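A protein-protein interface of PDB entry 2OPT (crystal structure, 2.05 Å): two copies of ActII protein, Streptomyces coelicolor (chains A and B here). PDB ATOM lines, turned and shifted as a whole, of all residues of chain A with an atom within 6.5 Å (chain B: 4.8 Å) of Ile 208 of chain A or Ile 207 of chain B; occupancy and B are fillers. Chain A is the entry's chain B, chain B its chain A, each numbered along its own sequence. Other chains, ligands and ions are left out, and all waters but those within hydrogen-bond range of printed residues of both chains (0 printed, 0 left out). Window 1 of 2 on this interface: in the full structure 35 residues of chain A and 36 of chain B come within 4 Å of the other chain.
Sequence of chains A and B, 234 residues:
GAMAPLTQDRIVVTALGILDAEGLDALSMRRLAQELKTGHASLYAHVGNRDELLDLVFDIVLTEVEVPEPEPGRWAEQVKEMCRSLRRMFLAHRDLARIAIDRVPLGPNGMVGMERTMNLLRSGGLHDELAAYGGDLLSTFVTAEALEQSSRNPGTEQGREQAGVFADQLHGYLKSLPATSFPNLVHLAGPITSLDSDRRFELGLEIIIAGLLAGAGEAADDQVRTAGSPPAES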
ATOM      1  N   LEU A 130     -37.492 -21.869   5.392  1.00  0.00           N
ATOM      2  CA  LEU A 130     -36.838 -21.302   6.554  1.00  0.00           C
ATOM      3  C   LEU A 130     -36.858 -22.258   7.739  1.00  0.00           C
ATOM      4  O   LEU A 130     -35.918 -22.321   8.523  1.00  0.00           O
ATOM      5  CB  LEU A 130     -37.563 -20.044   6.989  1.00  0.00           C
ATOM      6  CG  LEU A 130     -36.782 -18.811   7.419  1.00  0.00           C
ATOM      7  CD1 LEU A 130     -37.615 -17.768   8.234  1.00  0.00           C
ATOM      8  CD2 LEU A 130     -35.457 -19.107   8.034  1.00  0.00           C
ATOM      9  N   TYR A 133     -34.453 -25.300   6.597  1.00  0.00           N
ATOM     10  CA  TYR A 133     -33.061 -24.925   6.678  1.00  0.00           C
ATOM     11  C   TYR A 133     -32.618 -24.503   8.068  1.00  0.00           C
ATOM     12  O   TYR A 133     -31.490 -24.815   8.448  1.00  0.00           O
ATOM     13  CB  TYR A 133     -32.688 -23.813   5.699  1.00  0.00           C
ATOM     14  CG  TYR A 133     -31.206 -23.526   5.811  1.00  0.00           C
ATOM     15  CD1 TYR A 133     -30.279 -24.483   5.416  1.00  0.00           C
ATOM     16  CD2 TYR A 133     -30.725 -22.323   6.390  1.00  0.00           C
ATOM     17  CE1 TYR A 133     -28.915 -24.260   5.528  1.00  0.00           C
ATOM     18  CE2 TYR A 133     -29.363 -22.101   6.524  1.00  0.00           C
ATOM     19  CZ  TYR A 133     -28.461 -23.068   6.075  1.00  0.00           C
ATOM     20  OH  TYR A 133     -27.100 -22.891   6.163  1.00  0.00           O
ATOM     21  N   GLY A 134     -33.484 -23.808   8.823  1.00  0.00           N
ATOM     22  CA  GLY A 134     -33.114 -23.363  10.169  1.00  0.00           C
ATOM     23  C   GLY A 134     -32.917 -24.521  11.131  1.00  0.00           C
ATOM     24  O   GLY A 134     -32.038 -24.475  12.017  1.00  0.00           O
ATOM     25  N   LEU A 137     -29.385 -25.661  10.094  1.00  0.00           N
ATOM     26  CA  LEU A 137     -28.359 -24.745  10.579  1.00  0.00           C
ATOM     27  C   LEU A 137     -28.211 -24.876  12.071  1.00  0.00           C
ATOM     28  O   LEU A 137     -27.118 -24.829  12.560  1.00  0.00           O
ATOM     29  CB  LEU A 137     -28.704 -23.295  10.273  1.00  0.00           C
ATOM     30  CG  LEU A 137     -27.719 -22.157  10.627  1.00  0.00           C
ATOM     31  CD1 LEU A 137     -26.320 -22.360   9.965  1.00  0.00           C
ATOM     32  CD2 LEU A 137     -28.282 -20.837  10.133  1.00  0.00           C
ATOM     33  N   LEU A 138     -29.288 -24.959  12.810  1.00  0.00           N
ATOM     34  CA  LEU A 138     -29.104 -24.994  14.314  1.00  0.00           C
ATOM     35  C   LEU A 138     -28.418 -26.253  14.779  1.00  0.00           C
ATOM     36  O   LEU A 138     -27.618 -26.282  15.748  1.00  0.00           O
ATOM     37  CB  LEU A 138     -30.480 -24.950  14.957  1.00  0.00           C
ATOM     38  CG  LEU A 138     -31.199 -23.595  14.955  1.00  0.00           C
ATOM     39  CD1 LEU A 138     -32.644 -23.762  15.312  1.00  0.00           C
ATOM     40  CD2 LEU A 138     -30.498 -22.499  15.885  1.00  0.00           C
ATOM     41  N   PHE A 141     -24.789 -25.927  13.888  1.00  0.00           N
ATOM     42  CA  PHE A 141     -24.158 -25.027  14.848  1.00  0.00           C
ATOM     43  C   PHE A 141     -23.872 -25.744  16.152  1.00  0.00           C
ATOM     44  O   PHE A 141     -22.749 -25.686  16.714  1.00  0.00           O
ATOM     45  CB  PHE A 141     -25.086 -23.839  15.127  1.00  0.00           C
ATOM     46  CG  PHE A 141     -24.670 -23.045  16.327  1.00  0.00           C
ATOM     47  CD1 PHE A 141     -23.533 -22.232  16.267  1.00  0.00           C
ATOM     48  CD2 PHE A 141     -25.376 -23.138  17.517  1.00  0.00           C
ATOM     49  CE1 PHE A 141     -23.112 -21.500  17.350  1.00  0.00           C
ATOM     50  CE2 PHE A 141     -24.916 -22.446  18.666  1.00  0.00           C
ATOM     51  CZ  PHE A 141     -23.782 -21.637  18.570  1.00  0.00           C
ATOM     52  N   VAL A 142     -24.899 -26.367  16.718  1.00  0.00           N
ATOM     53  CA  VAL A 142     -24.691 -27.048  18.014  1.00  0.00           C
ATOM     54  C   VAL A 142     -23.588 -28.136  17.967  1.00  0.00           C
ATOM     55  O   VAL A 142     -22.734 -28.263  18.887  1.00  0.00           O
ATOM     56  CB  VAL A 142     -25.991 -27.623  18.565  1.00  0.00           C
ATOM     57  CG1 VAL A 142     -25.701 -28.385  19.858  1.00  0.00           C
ATOM     58  CG2 VAL A 142     -26.965 -26.513  18.796  1.00  0.00           C
ATOM     59  N   LEU A 203     -23.866 -16.909  22.420  1.00  0.00           N
ATOM     60  CA  LEU A 203     -23.808 -15.877  21.434  1.00  0.00           C
ATOM     61  C   LEU A 203     -24.318 -16.378  20.094  1.00  0.00           C
ATOM     62  O   LEU A 203     -25.156 -15.733  19.444  1.00  0.00           O
ATOM     63  CB  LEU A 203     -22.373 -15.360  21.254  1.00  0.00           C
ATOM     64  CG  LEU A 203     -22.059 -13.939  21.699  1.00  0.00           C
ATOM     65  CD1 LEU A 203     -20.595 -13.680  21.419  1.00  0.00           C
ATOM     66  CD2 LEU A 203     -22.967 -12.906  20.987  1.00  0.00           C
ATOM     67  N   GLY A 204     -23.755 -17.501  19.643  1.00  0.00           N
ATOM     68  CA  GLY A 204     -24.105 -18.083  18.346  1.00  0.00           C
ATOM     69  C   GLY A 204     -25.573 -18.481  18.335  1.00  0.00           C
ATOM     70  O   GLY A 204     -26.227 -18.281  17.357  1.00  0.00           O
ATOM     71  N   LEU A 205     -26.082 -19.045  19.445  1.00  0.00           N
ATOM     72  CA  LEU A 205     -27.475 -19.447  19.536  1.00  0.00           C
ATOM     73  C   LEU A 205     -28.441 -18.251  19.316  1.00  0.00           C
ATOM     74  O   LEU A 205     -29.391 -18.309  18.468  1.00  0.00           O
ATOM     75  CB  LEU A 205     -27.732 -20.082  20.943  1.00  0.00           C
ATOM     76  CG  LEU A 205     -28.583 -21.326  21.033  1.00  0.00           C
ATOM     77  CD1 LEU A 205     -29.030 -21.562  22.478  1.00  0.00           C
ATOM     78  CD2 LEU A 205     -29.728 -21.156  20.136  1.00  0.00           C
ATOM     79  N   GLU A 206     -28.170 -17.151  20.030  1.00  0.00           N
ATOM     80  CA  GLU A 206     -28.900 -15.876  19.861  1.00  0.00           C
ATOM     81  C   GLU A 206     -28.829 -15.301  18.447  1.00  0.00           C
ATOM     82  O   GLU A 206     -29.828 -14.831  17.926  1.00  0.00           O
ATOM     83  CB  GLU A 206     -28.410 -14.830  20.855  1.00  0.00           C
ATOM     84  CG  GLU A 206     -29.202 -13.490  20.890  1.00  0.00           C
ATOM     85  CD  GLU A 206     -30.697 -13.642  21.119  1.00  0.00           C
ATOM     86  OE1 GLU A 206     -31.131 -14.552  21.885  1.00  0.00           O
ATOM     87  OE2 GLU A 206     -31.452 -12.805  20.582  1.00  0.00           O
ATOM     88  N   ILE A 207     -27.634 -15.271  17.870  1.00  0.00           N
ATOM     89  CA  ILE A 207     -27.484 -14.788  16.537  1.00  0.00           C
ATOM     90  C   ILE A 207     -28.395 -15.558  15.604  1.00  0.00           C
ATOM     91  O   ILE A 207     -29.115 -14.934  14.833  1.00  0.00           O
ATOM     92  CB  ILE A 207     -26.002 -14.857  16.030  1.00  0.00           C
ATOM     93  CG1 ILE A 207     -25.136 -13.835  16.782  1.00  0.00           C
ATOM     94  CG2 ILE A 207     -25.951 -14.597  14.494  1.00  0.00           C
ATOM     95  CD1 ILE A 207     -23.596 -14.140  16.822  1.00  0.00           C
ATOM     96  N   ILE A 208     -28.371 -16.896  15.641  1.00  0.00           N
ATOM     97  CA  ILE A 208     -29.180 -17.700  14.693  1.00  0.00           C
ATOM     98  C   ILE A 208     -30.679 -17.538  14.940  1.00  0.00           C
ATOM     99  O   ILE A 208     -31.447 -17.267  14.026  1.00  0.00           O
ATOM    100  CB  ILE A 208     -28.800 -19.180  14.722  1.00  0.00           C
ATOM    101  CG1 ILE A 208     -27.363 -19.368  14.175  1.00  0.00           C
ATOM    102  CG2 ILE A 208     -29.844 -20.057  13.874  1.00  0.00           C
ATOM    103  CD1 ILE A 208     -26.721 -20.688  14.633  1.00  0.00           C
ATOM    104  N   ILE A 209     -31.074 -17.619  16.193  1.00  0.00           N
ATOM    105  CA  ILE A 209     -32.463 -17.352  16.563  1.00  0.00           C
ATOM    106  C   ILE A 209     -33.013 -15.965  16.171  1.00  0.00           C
ATOM    107  O   ILE A 209     -34.095 -15.892  15.590  1.00  0.00           O
ATOM    108  CB  ILE A 209     -32.683 -17.513  18.044  1.00  0.00           C
ATOM    109  CG1 ILE A 209     -32.420 -18.954  18.485  1.00  0.00           C
ATOM    110  CG2 ILE A 209     -34.116 -17.108  18.393  1.00  0.00           C
ATOM    111  CD1 ILE A 209     -33.519 -19.875  18.147  1.00  0.00           C
ATOM    112  N   ALA A 210     -32.269 -14.891  16.473  1.00  0.00           N
ATOM    113  CA  ALA A 210     -32.609 -13.542  16.038  1.00  0.00           C
ATOM    114  C   ALA A 210     -32.746 -13.460  14.497  1.00  0.00           C
ATOM    115  O   ALA A 210     -33.657 -12.842  13.975  1.00  0.00           O
ATOM    116  CB  ALA A 210     -31.574 -12.503  16.567  1.00  0.00           C
ATOM    117  N   GLY A 211     -31.873 -14.136  13.784  1.00  0.00           N
ATOM    118  CA  GLY A 211     -31.912 -14.087  12.314  1.00  0.00           C
ATOM    119  C   GLY A 211     -33.051 -14.921  11.746  1.00  0.00           C
ATOM    120  O   GLY A 211     -33.576 -14.600  10.686  1.00  0.00           O
ATOM    121  N   LEU A 212     -33.392 -16.034  12.388  1.00  0.00           N
ATOM    122  CA  LEU A 212     -34.609 -16.766  11.993  1.00  0.00           C
ATOM    123  C   LEU A 212     -35.857 -15.931  12.236  1.00  0.00           C
ATOM    124  O   LEU A 212     -36.771 -15.915  11.385  1.00  0.00           O
ATOM    125  CB  LEU A 212     -34.758 -18.111  12.761  1.00  0.00           C
ATOM    126  CG  LEU A 212     -33.636 -19.118  12.465  1.00  0.00           C
ATOM    127  CD1 LEU A 212     -33.768 -20.286  13.397  1.00  0.00           C
ATOM    128  CD2 LEU A 212     -33.748 -19.586  11.003  1.00  0.00           C
ATOM    129  N   LEU A 213     -35.911 -15.256  13.390  1.00  0.00           N
ATOM    130  CA  LEU A 213     -37.064 -14.399  13.682  1.00  0.00           C
ATOM    131  C   LEU A 213     -37.170 -13.291  12.650  1.00  0.00           C
ATOM    132  O   LEU A 213     -38.263 -12.981  12.179  1.00  0.00           O
ATOM    133  CB  LEU A 213     -36.975 -13.769  15.070  1.00  0.00           C
ATOM    134  CG  LEU A 213     -37.208 -14.687  16.259  1.00  0.00           C
ATOM    135  CD1 LEU A 213     -36.756 -13.969  17.507  1.00  0.00           C
ATOM    136  CD2 LEU A 213     -38.665 -15.060  16.361  1.00  0.00           C
ATOM    137  N   ALA A 214     -36.032 -12.672  12.325  1.00  0.00           N
ATOM    138  CA  ALA A 214     -36.004 -11.659  11.295  1.00  0.00           C
ATOM    139  C   ALA A 214     -36.549 -12.175   9.970  1.00  0.00           C
ATOM    140  O   ALA A 214     -37.279 -11.464   9.292  1.00  0.00           O
ATOM    141  CB  ALA A 214     -34.586 -11.140  11.113  1.00  0.00           C
ATOM    142  N   GLY A 215     -36.170 -13.391   9.585  1.00  0.00           N
ATOM    143  CA  GLY A 215     -36.616 -14.007   8.339  1.00  0.00           C
ATOM    144  C   GLY A 215     -38.095 -14.334   8.350  1.00  0.00           C
ATOM    145  O   GLY A 215     -38.758 -14.299   7.307  1.00  0.00           O
ATOM    146  N   LEU B 137     -18.065 -17.433  13.189  1.00  0.00           N
ATOM    147  CA  LEU B 137     -19.296 -18.109  12.854  1.00  0.00           C
ATOM    148  C   LEU B 137     -19.521 -17.973  11.333  1.00  0.00           C
ATOM    149  O   LEU B 137     -19.943 -18.897  10.664  1.00  0.00           O
ATOM    150  CB  LEU B 137     -20.495 -17.511  13.639  1.00  0.00           C
ATOM    151  CG  LEU B 137     -21.896 -18.062  13.236  1.00  0.00           C
ATOM    152  CD1 LEU B 137     -21.925 -19.541  13.525  1.00  0.00           C
ATOM    153  CD2 LEU B 137     -23.129 -17.385  13.893  1.00  0.00           C
ATOM    154  N   LEU B 203     -29.852 -18.359   2.367  1.00  0.00           N
ATOM    155  CA  LEU B 203     -30.643 -18.371   3.585  1.00  0.00           C
ATOM    156  C   LEU B 203     -29.759 -18.289   4.818  1.00  0.00           C
ATOM    157  O   LEU B 203     -30.031 -17.484   5.705  1.00  0.00           O
ATOM    158  CB  LEU B 203     -31.492 -19.661   3.698  1.00  0.00           C
ATOM    159  CG  LEU B 203     -32.855 -19.655   3.068  1.00  0.00           C
ATOM    160  CD1 LEU B 203     -33.528 -21.054   3.107  1.00  0.00           C
ATOM    161  CD2 LEU B 203     -33.720 -18.614   3.809  1.00  0.00           C
ATOM    162  N   GLY B 204     -28.734 -19.129   4.918  1.00  0.00           N
ATOM    163  CA  GLY B 204     -27.872 -19.105   6.131  1.00  0.00           C
ATOM    164  C   GLY B 204     -27.136 -17.773   6.249  1.00  0.00           C
ATOM    165  O   GLY B 204     -26.930 -17.260   7.328  1.00  0.00           O
ATOM    166  N   LEU B 205     -26.658 -17.222   5.126  1.00  0.00           N
ATOM    167  CA  LEU B 205     -26.081 -15.880   5.138  1.00  0.00           C
ATOM    168  C   LEU B 205     -27.065 -14.821   5.702  1.00  0.00           C
ATOM    169  O   LEU B 205     -26.701 -14.064   6.561  1.00  0.00           O
ATOM    170  CB  LEU B 205     -25.647 -15.502   3.687  1.00  0.00           C
ATOM    171  CG  LEU B 205     -24.431 -14.642   3.459  1.00  0.00           C
ATOM    172  CD1 LEU B 205     -23.283 -15.127   4.291  1.00  0.00           C
ATOM    173  CD2 LEU B 205     -24.089 -14.628   1.900  1.00  0.00           C
ATOM    174  N   GLU B 206     -28.295 -14.791   5.178  1.00  0.00           N
ATOM    175  CA  GLU B 206     -29.337 -13.861   5.622  1.00  0.00           C
ATOM    176  C   GLU B 206     -29.541 -13.994   7.120  1.00  0.00           C
ATOM    177  O   GLU B 206     -29.531 -12.998   7.860  1.00  0.00           O
ATOM    178  CB  GLU B 206     -30.645 -14.184   4.887  1.00  0.00           C
ATOM    179  CG  GLU B 206     -30.667 -13.634   3.464  1.00  0.00           C
ATOM    180  CD  GLU B 206     -31.913 -13.970   2.667  1.00  0.00           C
ATOM    181  OE1 GLU B 206     -32.881 -14.591   3.209  1.00  0.00           O
ATOM    182  OE2 GLU B 206     -31.917 -13.585   1.468  1.00  0.00           O
ATOM    183  N   ILE B 207     -29.702 -15.240   7.561  1.00  0.00           N
ATOM    184  CA  ILE B 207     -29.967 -15.528   8.943  1.00  0.00           C
ATOM    185  C   ILE B 207     -28.862 -14.959   9.829  1.00  0.00           C
ATOM    186  O   ILE B 207     -29.149 -14.266  10.784  1.00  0.00           O
ATOM    187  CB  ILE B 207     -30.158 -17.037   9.189  1.00  0.00           C
ATOM    188  CG1 ILE B 207     -31.471 -17.512   8.535  1.00  0.00           C
ATOM    189  CG2 ILE B 207     -30.150 -17.338  10.670  1.00  0.00           C
ATOM    190  CD1 ILE B 207     -31.613 -19.005   8.399  1.00  0.00           C
ATOM    191  N   ILE B 208     -27.604 -15.284   9.521  1.00  0.00           N
ATOM    192  CA  ILE B 208     -26.464 -14.887  10.400  1.00  0.00           C
ATOM    193  C   ILE B 208     -26.286 -13.367  10.418  1.00  0.00           C
ATOM    194  O   ILE B 208     -26.083 -12.788  11.471  1.00  0.00           O
ATOM    195  CB  ILE B 208     -25.152 -15.563   9.950  1.00  0.00           C
ATOM    196  CG1 ILE B 208     -25.298 -17.095  10.079  1.00  0.00           C
ATOM    197  CG2 ILE B 208     -23.943 -14.934  10.680  1.00  0.00           C
ATOM    198  CD1 ILE B 208     -24.162 -17.979   9.440  1.00  0.00           C
ATOM    199  N   ILE B 209     -26.402 -12.733   9.250  1.00  0.00           N
ATOM    200  CA  ILE B 209     -26.256 -11.256   9.122  1.00  0.00           C
ATOM    201  C   ILE B 209     -27.392 -10.533   9.889  1.00  0.00           C
ATOM    202  O   ILE B 209     -27.119  -9.626  10.692  1.00  0.00           O
ATOM    203  CB  ILE B 209     -26.179 -10.851   7.625  1.00  0.00           C
ATOM    204  CG1 ILE B 209     -24.835 -11.298   7.021  1.00  0.00           C
ATOM    205  CG2 ILE B 209     -26.235  -9.321   7.452  1.00  0.00           C
ATOM    206  CD1 ILE B 209     -24.869 -11.290   5.557  1.00  0.00           C
ATOM    207  N   ALA B 210     -28.652 -10.944   9.699  1.00  0.00           N
ATOM    208  CA  ALA B 210     -29.739 -10.379  10.486  1.00  0.00           C
ATOM    209  C   ALA B 210     -29.465 -10.541  12.001  1.00  0.00           C
ATOM    210  O   ALA B 210     -29.730  -9.649  12.787  1.00  0.00           O
ATOM    211  CB  ALA B 210     -31.114 -11.054  10.135  1.00  0.00           C
ATOM    212  N   GLY B 211     -28.941 -11.680  12.406  1.00  0.00           N
ATOM    213  CA  GLY B 211     -28.761 -11.951  13.857  1.00  0.00           C
ATOM    214  C   GLY B 211     -27.625 -11.116  14.382  1.00  0.00           C
ATOM    215  O   GLY B 211     -27.655 -10.687  15.508  1.00  0.00           O
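Among the printed residues, merely in contact across the chains: Leu 130 of chain A with Ile 207 of chain B, Tyr 133 of chain A with Leu 203 of chain B, Tyr 133 of chain A with Gly 204 of chain B, Tyr 133 of chain A with Ile 207 of chain B, Ile 207 of chain A with Ile 208 of chain B, Ile 207 of chain A with Gly 211 of chain B, Ile 208 of chain A with Ile 207 of chain B, Ala 210 of chain A with Gly 211 of chain B, Gly 211 of chain A with Ile 207 of chain B, Gly 211 of chain A with Ala 210 of chain B, Gly 211 of chain A with Gly 211 of chain B, Leu 212 of chain A with Ile 207 of chain B and Ala 214 of chain A with Ala 210 of chain B.
Of chain B, only Ile 207 (3.6 Å) comes within 4 Å of Ile 208 of chain A. Of the printed residues of chain B, Ala 210 of chain A touches Gly 211 (3.9 Å). Printed residues of chain B within 4 Å of Leu 212 of chain A: Ile 207. The nearest printed residue of chain A that does not touch Ile 207 of chain B is Leu 137 of chain A (4.003 Å).
Of the 10 printed residues of chain B, 6 touch a printed residue of chain A. Of the 20 printed residues of chain A, 8 touch a printed residue of chain B.
Ile 207 of chain A touches Ile 208 of chain B, and with the chains exchanged Ile 208 of chain A touches Ile 207 of chain B. Ile 207 of chain A touches Gly 211 of chain B, and with the chains exchanged Gly 211 of chain A touches Ile 207 of chain B. Ala 210 of chain A touches Gly 211 of chain B, and with the chains exchanged Gly 211 of chain A touches Ala 210 of chain B. Gly 211 of chain A touches its own counterpart, Gly 211 of chain B. Of the 13 pairs that touch across the chains among the printed residues, 7 have their exchanged pair printed and touching as well.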
